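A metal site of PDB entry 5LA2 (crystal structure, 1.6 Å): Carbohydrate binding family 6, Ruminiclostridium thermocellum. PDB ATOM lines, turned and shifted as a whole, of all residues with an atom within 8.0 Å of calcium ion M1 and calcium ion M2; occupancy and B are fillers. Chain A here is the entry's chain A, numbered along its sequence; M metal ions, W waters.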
ATOM      1  N   ASN A 353       8.732 -23.774 -13.864  1.00  0.00           N
ATOM      2  CA  ASN A 353       8.073 -22.504 -14.135  1.00  0.00           C
ATOM      3  C   ASN A 353       6.551 -22.682 -14.128  1.00  0.00           C
ATOM      4  O   ASN A 353       5.987 -23.635 -14.705  1.00  0.00           O
ATOM      5  CB  ASN A 353       8.608 -21.913 -15.460  1.00  0.00           C
ATOM      6  CG  ASN A 353       8.414 -20.424 -15.566  1.00  0.00           C
ATOM      7  OD1 ASN A 353       8.073 -19.761 -14.611  1.00  0.00           O
ATOM      8  ND2 ASN A 353       8.657 -19.891 -16.762  1.00  0.00           N
ATOM      9  N   TYR A 357       8.094 -21.824  -9.106  1.00  0.00           N
ATOM     10  CA  TYR A 357       8.435 -20.415  -9.287  1.00  0.00           C
ATOM     11  C   TYR A 357       7.772 -19.945 -10.562  1.00  0.00           C
ATOM     12  O   TYR A 357       7.294 -20.743 -11.345  1.00  0.00           O
ATOM     13  CB  TYR A 357       9.941 -20.258  -9.421  1.00  0.00           C
ATOM     14  CG  TYR A 357      10.533 -20.959 -10.626  1.00  0.00           C
ATOM     15  CD1 TYR A 357      10.642 -20.310 -11.854  1.00  0.00           C
ATOM     16  CD2 TYR A 357      11.015 -22.276 -10.522  1.00  0.00           C
ATOM     17  CE1 TYR A 357      11.218 -20.950 -12.960  1.00  0.00           C
ATOM     18  CE2 TYR A 357      11.595 -22.918 -11.621  1.00  0.00           C
ATOM     19  CZ  TYR A 357      11.675 -22.250 -12.837  1.00  0.00           C
ATOM     20  OH  TYR A 357      12.254 -22.890 -13.898  1.00  0.00           O
ATOM     21  N   TYR A 358       7.788 -18.647 -10.775  1.00  0.00           N
ATOM     22  CA  TYR A 358       7.496 -18.069 -12.060  1.00  0.00           C
ATOM     23  C   TYR A 358       8.605 -17.068 -12.362  1.00  0.00           C
ATOM     24  O   TYR A 358       8.836 -16.115 -11.579  1.00  0.00           O
ATOM     25  CB  TYR A 358       6.129 -17.388 -12.077  1.00  0.00           C
ATOM     26  CG  TYR A 358       5.922 -16.456 -13.265  1.00  0.00           C
ATOM     27  CD1 TYR A 358       6.239 -16.855 -14.572  1.00  0.00           C
ATOM     28  CD2 TYR A 358       5.424 -15.185 -13.070  1.00  0.00           C
ATOM     29  CE1 TYR A 358       6.057 -16.000 -15.652  1.00  0.00           C
ATOM     30  CE2 TYR A 358       5.225 -14.332 -14.139  1.00  0.00           C
ATOM     31  CZ  TYR A 358       5.558 -14.727 -15.419  1.00  0.00           C
ATOM     32  OH  TYR A 358       5.347 -13.868 -16.467  1.00  0.00           O
ATOM     33  N   ASP A 359       9.304 -17.325 -13.460  1.00  0.00           N
ATOM     34  CA  ASP A 359      10.239 -16.364 -14.002  1.00  0.00           C
ATOM     35  C   ASP A 359       9.834 -15.931 -15.398  1.00  0.00           C
ATOM     36  O   ASP A 359       9.346 -16.759 -16.183  1.00  0.00           O
ATOM     37  CB  ASP A 359      11.659 -16.939 -14.016  1.00  0.00           C
ATOM     38  CG  ASP A 359      12.676 -15.849 -13.913  1.00  0.00           C
ATOM     39  OD1 ASP A 359      13.004 -15.475 -12.760  1.00  0.00           O
ATOM     40  OD2 ASP A 359      13.155 -15.346 -14.973  1.00  0.00           O
ATOM     41  N   THR A 360      10.044 -14.662 -15.702  1.00  0.00           N
ATOM     42  CA  THR A 360       9.568 -14.088 -16.982  1.00  0.00           C
ATOM     43  C   THR A 360      10.335 -14.555 -18.212  1.00  0.00           C
ATOM     44  O   THR A 360       9.816 -14.458 -19.322  1.00  0.00           O
ATOM     45  CB  THR A 360       9.608 -12.551 -16.981  1.00  0.00           C
ATOM     46  OG1 THR A 360      10.958 -12.106 -16.767  1.00  0.00           O
ATOM     47  CG2 THR A 360       8.663 -11.997 -15.919  1.00  0.00           C
ATOM     48  N   ASP A 361      11.540 -15.061 -18.027  1.00  0.00           N
ATOM     49  CA  ASP A 361      12.302 -15.694 -19.115  1.00  0.00           C
ATOM     50  C   ASP A 361      12.879 -17.006 -18.636  1.00  0.00           C
ATOM     51  O   ASP A 361      13.315 -17.109 -17.489  1.00  0.00           O
ATOM     52  CB  ASP A 361      13.356 -14.763 -19.774  1.00  0.00           C
ATOM     53  CG  ASP A 361      14.195 -13.957 -18.779  1.00  0.00           C
ATOM     54  OD1 ASP A 361      14.565 -14.461 -17.704  1.00  0.00           O
ATOM     55  OD2 ASP A 361      14.530 -12.792 -19.102  1.00  0.00           O
ATOM     56  N   SER A 362      12.872 -18.023 -19.501  1.00  0.00           N
ATOM     57  CA  SER A 362      13.292 -19.348 -19.073  1.00  0.00           C
ATOM     58  C   SER A 362      14.816 -19.463 -18.962  1.00  0.00           C
ATOM     59  O   SER A 362      15.308 -20.344 -18.286  1.00  0.00           O
ATOM     60  CB  SER A 362      12.749 -20.408 -20.002  1.00  0.00           C
ATOM     61  OG  SER A 362      13.198 -20.152 -21.286  1.00  0.00           O
ATOM     62  N   VAL A 363      15.564 -18.592 -19.615  1.00  0.00           N
ATOM     63  CA  VAL A 363      17.011 -18.541 -19.355  1.00  0.00           C
ATOM     64  C   VAL A 363      17.282 -18.110 -17.899  1.00  0.00           C
ATOM     65  O   VAL A 363      16.534 -17.320 -17.333  1.00  0.00           O
ATOM     66  CB  VAL A 363      17.718 -17.589 -20.359  1.00  0.00           C
ATOM     67  CG1 VAL A 363      17.350 -16.140 -20.115  1.00  0.00           C
ATOM     68  CG2 VAL A 363      19.232 -17.796 -20.338  1.00  0.00           C
ATOM     69  N   ASN A 364      18.316 -18.673 -17.286  1.00  0.00           N
ATOM     70  CA  ASN A 364      18.867 -18.144 -16.050  1.00  0.00           C
ATOM     71  C   ASN A 364      19.937 -17.118 -16.454  1.00  0.00           C
ATOM     72  O   ASN A 364      21.071 -17.476 -16.778  1.00  0.00           O
ATOM     73  CB  ASN A 364      19.440 -19.295 -15.240  1.00  0.00           C
ATOM     74  CG  ASN A 364      20.204 -18.836 -14.009  1.00  0.00           C
ATOM     75  OD1 ASN A 364      20.497 -17.648 -13.832  1.00  0.00           O
ATOM     76  ND2 ASN A 364      20.560 -19.786 -13.182  1.00  0.00           N
ATOM     77  N   VAL A 365      19.601 -15.839 -16.417  1.00  0.00           N
ATOM     78  CA  VAL A 365      20.490 -14.815 -17.046  1.00  0.00           C
ATOM     79  C   VAL A 365      21.843 -14.699 -16.327  1.00  0.00           C
ATOM     80  O   VAL A 365      22.877 -14.503 -16.954  1.00  0.00           O
ATOM     81  CB  VAL A 365      19.819 -13.421 -17.182  1.00  0.00           C
ATOM     82  CG1 VAL A 365      18.477 -13.478 -17.893  1.00  0.00           C
ATOM     83  CG2 VAL A 365      19.598 -12.805 -15.856  1.00  0.00           C
ATOM     84  N   GLY A 366      21.840 -14.851 -15.005  1.00  0.00           N
ATOM     85  CA  GLY A 366      23.080 -14.893 -14.243  1.00  0.00           C
ATOM     86  C   GLY A 366      23.915 -16.136 -14.496  1.00  0.00           C
ATOM     87  O   GLY A 366      25.135 -16.111 -14.307  1.00  0.00           O
ATOM     88  N   GLU A 373      17.142 -24.079 -14.709  1.00  0.00           N
ATOM     89  CA  GLU A 373      15.851 -23.498 -14.341  1.00  0.00           C
ATOM     90  C   GLU A 373      15.839 -21.997 -14.629  1.00  0.00           C
ATOM     91  O   GLU A 373      16.857 -21.392 -14.927  1.00  0.00           O
ATOM     92  CB  GLU A 373      15.546 -23.800 -12.881  1.00  0.00           C
ATOM     93  CG  GLU A 373      15.311 -25.277 -12.651  1.00  0.00           C
ATOM     94  CD  GLU A 373      15.596 -25.699 -11.237  1.00  0.00           C
ATOM     95  OE1 GLU A 373      16.794 -25.884 -10.883  1.00  0.00           O
ATOM     96  OE2 GLU A 373      14.624 -25.854 -10.482  1.00  0.00           O
ATOM     97  N   GLY A 374      14.660 -21.401 -14.579  1.00  0.00           N
ATOM     98  CA  GLY A 374      14.463 -20.059 -15.081  1.00  0.00           C
ATOM     99  C   GLY A 374      14.771 -18.918 -14.143  1.00  0.00           C
ATOM    100  O   GLY A 374      14.845 -17.779 -14.575  1.00  0.00           O
ATOM    101  N   VAL A 375      14.923 -19.213 -12.856  1.00  0.00           N
ATOM    102  CA  VAL A 375      15.208 -18.160 -11.889  1.00  0.00           C
ATOM    103  C   VAL A 375      16.606 -17.599 -12.204  1.00  0.00           C
ATOM    104  O   VAL A 375      17.518 -18.334 -12.545  1.00  0.00           O
ATOM    105  CB  VAL A 375      15.115 -18.691 -10.461  1.00  0.00           C
ATOM    106  CG1 VAL A 375      15.477 -17.613  -9.440  1.00  0.00           C
ATOM    107  CG2 VAL A 375      13.714 -19.263 -10.232  1.00  0.00           C
ATOM    108  N   ASP A 376      16.751 -16.281 -12.119  1.00  0.00           N
ATOM    109  CA  ASP A 376      18.013 -15.644 -12.474  1.00  0.00           C
ATOM    110  C   ASP A 376      18.889 -15.528 -11.243  1.00  0.00           C
ATOM    111  O   ASP A 376      18.495 -14.864 -10.279  1.00  0.00           O
ATOM    112  CB  ASP A 376      17.736 -14.285 -13.128  1.00  0.00           C
ATOM    113  CG  ASP A 376      16.775 -14.432 -14.290  1.00  0.00           C
ATOM    114  OD1 ASP A 376      17.054 -15.316 -15.166  1.00  0.00           O
ATOM    115  OD2 ASP A 376      15.692 -13.789 -14.287  1.00  0.00           O
ATOM    116  N   ILE A 377      20.042 -16.201 -11.309  1.00  0.00           N
ATOM    117  CA  ILE A 377      20.914 -16.389 -10.188  1.00  0.00           C
ATOM    118  C   ILE A 377      22.364 -16.011 -10.521  1.00  0.00           C
ATOM    119  O   ILE A 377      22.908 -16.489 -11.520  1.00  0.00           O
ATOM    120  CB  ILE A 377      20.882 -17.831  -9.653  1.00  0.00           C
ATOM    121  CG1 ILE A 377      19.449 -18.313  -9.405  1.00  0.00           C
ATOM    122  CG2 ILE A 377      21.613 -17.906  -8.321  1.00  0.00           C
ATOM    123  CD1 ILE A 377      19.347 -19.795  -9.090  1.00  0.00           C
ATOM    124  N   VAL A 389      19.376 -14.300  -5.920  1.00  0.00           N
ATOM    125  CA  VAL A 389      18.467 -14.162  -6.994  1.00  0.00           C
ATOM    126  C   VAL A 389      18.469 -12.692  -7.419  1.00  0.00           C
ATOM    127  O   VAL A 389      18.406 -11.788  -6.587  1.00  0.00           O
ATOM    128  CB  VAL A 389      17.036 -14.600  -6.579  1.00  0.00           C
ATOM    129  CG1 VAL A 389      16.069 -14.320  -7.727  1.00  0.00           C
ATOM    130  CG2 VAL A 389      17.034 -16.081  -6.194  1.00  0.00           C
ATOM    131  N   GLY A 390      18.546 -12.486  -8.726  1.00  0.00           N
ATOM    132  CA  GLY A 390      18.605 -11.182  -9.336  1.00  0.00           C
ATOM    133  C   GLY A 390      17.649 -11.125 -10.498  1.00  0.00           C
ATOM    134  O   GLY A 390      16.935 -12.096 -10.782  1.00  0.00           O
ATOM    135  N   TRP A 391      17.662 -10.012 -11.212  1.00  0.00           N
ATOM    136  CA  TRP A 391      16.708  -9.807 -12.350  1.00  0.00           C
ATOM    137  C   TRP A 391      15.298 -10.240 -11.959  1.00  0.00           C
ATOM    138  O   TRP A 391      14.672 -11.059 -12.620  1.00  0.00           O
ATOM    139  CB  TRP A 391      17.132 -10.569 -13.610  1.00  0.00           C
ATOM    140  CG  TRP A 391      18.495 -10.190 -14.070  1.00  0.00           C
ATOM    141  CD1 TRP A 391      18.812  -9.266 -15.007  1.00  0.00           C
ATOM    142  CD2 TRP A 391      19.747 -10.742 -13.600  1.00  0.00           C
ATOM    143  NE1 TRP A 391      20.176  -9.228 -15.181  1.00  0.00           N
ATOM    144  CE2 TRP A 391      20.770 -10.115 -14.316  1.00  0.00           C
ATOM    145  CE3 TRP A 391      20.083 -11.724 -12.672  1.00  0.00           C
ATOM    146  CZ2 TRP A 391      22.128 -10.419 -14.103  1.00  0.00           C
ATOM    147  CZ3 TRP A 391      21.418 -12.037 -12.459  1.00  0.00           C
ATOM    148  CH2 TRP A 391      22.429 -11.380 -13.172  1.00  0.00           C
ATOM    149  N   ILE A 392      14.846  -9.731 -10.841  1.00  0.00           N
ATOM    150  CA  ILE A 392      13.521 -10.033 -10.326  1.00  0.00           C
ATOM    151  C   ILE A 392      12.622  -8.995 -10.975  1.00  0.00           C
ATOM    152  O   ILE A 392      12.840  -7.796 -10.784  1.00  0.00           O
ATOM    153  CB  ILE A 392      13.461  -9.929  -8.807  1.00  0.00           C
ATOM    154  CG1 ILE A 392      14.438 -10.909  -8.155  1.00  0.00           C
ATOM    155  CG2 ILE A 392      12.031 -10.207  -8.329  1.00  0.00           C
ATOM    156  CD1 ILE A 392      14.362 -10.940  -6.625  1.00  0.00           C
ATOM    157  N   SER A 393      11.655  -9.491 -11.728  1.00  0.00           N
ATOM    158  CA  SER A 393      10.697  -8.686 -12.472  1.00  0.00           C
ATOM    159  C   SER A 393       9.307  -8.741 -11.854  1.00  0.00           C
ATOM    160  O   SER A 393       8.913  -9.723 -11.232  1.00  0.00           O
ATOM    161  CB  SER A 393      10.634  -9.217 -13.890  1.00  0.00           C
ATOM    162  OG  SER A 393      11.950  -9.135 -14.431  1.00  0.00           O
ATOM    163  N   GLU A 394       8.563  -7.665 -12.061  1.00  0.00           N
ATOM    164  CA  GLU A 394       7.207  -7.548 -11.577  1.00  0.00           C
ATOM    165  C   GLU A 394       6.387  -8.790 -11.959  1.00  0.00           C
ATOM    166  O   GLU A 394       6.443  -9.253 -13.109  1.00  0.00           O
ATOM    167  CB  GLU A 394       6.593  -6.271 -12.162  1.00  0.00           C
ATOM    168  CG  GLU A 394       5.180  -5.990 -11.710  1.00  0.00           C
ATOM    169  CD  GLU A 394       4.529  -4.866 -12.479  1.00  0.00           C
ATOM    170  OE1 GLU A 394       5.151  -4.287 -13.404  1.00  0.00           O
ATOM    171  OE2 GLU A 394       3.371  -4.560 -12.142  1.00  0.00           O
ATOM    172  N   GLU A 396       6.884 -11.887 -10.822  1.00  0.00           N
ATOM    173  CA  GLU A 396       7.611 -13.089 -10.504  1.00  0.00           C
ATOM    174  C   GLU A 396       7.289 -13.577  -9.081  1.00  0.00           C
ATOM    175  O   GLU A 396       6.837 -12.820  -8.201  1.00  0.00           O
ATOM    176  CB  GLU A 396       9.112 -12.873 -10.717  1.00  0.00           C
ATOM    177  CG  GLU A 396       9.454 -12.816 -12.190  1.00  0.00           C
ATOM    178  CD  GLU A 396      10.931 -12.845 -12.498  1.00  0.00           C
ATOM    179  OE1 GLU A 396      11.782 -12.523 -11.632  1.00  0.00           O
ATOM    180  OE2 GLU A 396      11.270 -13.202 -13.627  1.00  0.00           O
ATOM    181  N   TRP A 397       7.488 -14.872  -8.880  1.00  0.00           N
ATOM    182  CA  TRP A 397       7.347 -15.469  -7.560  1.00  0.00           C
ATOM    183  C   TRP A 397       8.223 -16.706  -7.391  1.00  0.00           C
ATOM    184  O   TRP A 397       8.677 -17.289  -8.361  1.00  0.00           O
ATOM    185  CB  TRP A 397       5.880 -15.780  -7.248  1.00  0.00           C
ATOM    186  CG  TRP A 397       5.091 -16.511  -8.266  1.00  0.00           C
ATOM    187  CD1 TRP A 397       4.283 -15.953  -9.225  1.00  0.00           C
ATOM    188  CD2 TRP A 397       4.939 -17.941  -8.400  1.00  0.00           C
ATOM    189  NE1 TRP A 397       3.653 -16.934  -9.936  1.00  0.00           N
ATOM    190  CE2 TRP A 397       4.048 -18.167  -9.457  1.00  0.00           C
ATOM    191  CE3 TRP A 397       5.458 -19.042  -7.712  1.00  0.00           C
ATOM    192  CZ2 TRP A 397       3.658 -19.436  -9.848  1.00  0.00           C
ATOM    193  CZ3 TRP A 397       5.100 -20.292  -8.105  1.00  0.00           C
ATOM    194  CH2 TRP A 397       4.199 -20.494  -9.174  1.00  0.00           C
ATOM    195  N   LEU A 398       8.503 -17.012  -6.126  1.00  0.00           N
ATOM    196  CA  LEU A 398       9.383 -18.083  -5.690  1.00  0.00           C
ATOM    197  C   LEU A 398       8.750 -18.755  -4.482  1.00  0.00           C
ATOM    198  O   LEU A 398       8.264 -18.079  -3.553  1.00  0.00           O
ATOM    199  CB  LEU A 398      10.723 -17.500  -5.218  1.00  0.00           C
ATOM    200  CG  LEU A 398      11.479 -16.681  -6.237  1.00  0.00           C
ATOM    201  CD1 LEU A 398      12.411 -15.684  -5.565  1.00  0.00           C
ATOM    202  CD2 LEU A 398      12.222 -17.601  -7.182  1.00  0.00           C
HETATM  203 CA    CA M   1      15.002 -16.059 -16.152  1.00  0.00          CA
HETATM  204 CA    CA M   2      13.714 -13.183 -13.247  1.00  0.00          CA
HETATM  205  O   HOH W   1      14.914 -13.915 -11.227  1.00  0.00           O
HETATM  206  O   HOH W   2      13.253 -11.816 -15.227  1.00  0.00           O
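The backbone carbonyl oxygen of Asp 376 is in hydrogen-bond range of the backbone NH of Gly 390 (2.8 Å).
N of Ser 393 sits close to OE1 of Glu 396.
N of Thr 360 lies close to OE2 of Glu 396 (2.8 Å).
The side-chain amide oxygen (OD1) of Asn 353 sits at hydrogen-bond distance from the backbone NH (N) of Asp 359, at 3.0 Å.
The backbone NH (N) of Gly 374 is in hydrogen-bond range of the side-chain hydroxyl (OH) of Tyr 357, 2.9 Å away.
The side-chain carboxylate (OD1) of Asp 376 lies close to the backbone NH (N) of Val 365, 2.9 Å away.
Of the 25 residues printed, 5 come within 4 Å of calcium ion M1.
Within 4 Å of calcium ion M2: Asp 359, Asp 376, Trp 391 and Glu 396.
The nearest printed residue that does not touch calcium ion M2 is Gly 390 (4.2 Å).
Calcium ion M1 is bound by OD1 of Asp 361 (2.3 Å), OD2 of Asp 359 (2.3 Å), O of Val 363 (2.3 Å), O of Gly 374 (2.3 Å), O of Asp 361 (2.4 Å) and OD1 of Asp 376 (2.4 Å).
Calcium ion M1 has six donor atoms within binding distance.
Slightly farther from calcium ion M1 lies the side-chain carboxylate (OD2) of Asp 376 (3.0 Å).
Calcium ion M2 is bound by the side-chain carboxylate (OD2) of Asp 376 (2.3 Å), the backbone carbonyl oxygen (O) of Trp 391 (2.4 Å), the side-chain carboxylate (OD1) of Asp 359 (2.4 Å), water W2 (2.4 Å), water W1 (2.5 Å), the side-chain carboxylate (OE2) of Glu 396 (2.5 Å), the side-chain carboxylate (OE1) of Glu 396 (2.6 Å) and the side-chain carboxylate (OD2) of Asp 359 (2.8 Å).
Water W1 lies within hydrogen-bond range of the backbone carbonyl oxygen (O) of Gly 390 (2.8 Å) and the backbone NH (N) of Asp 376 (3.1 Å).
Water W2 lies within hydrogen-bond range of OG1 of Thr 360 (2.8 Å) and OG of Ser 393 (3.1 Å).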
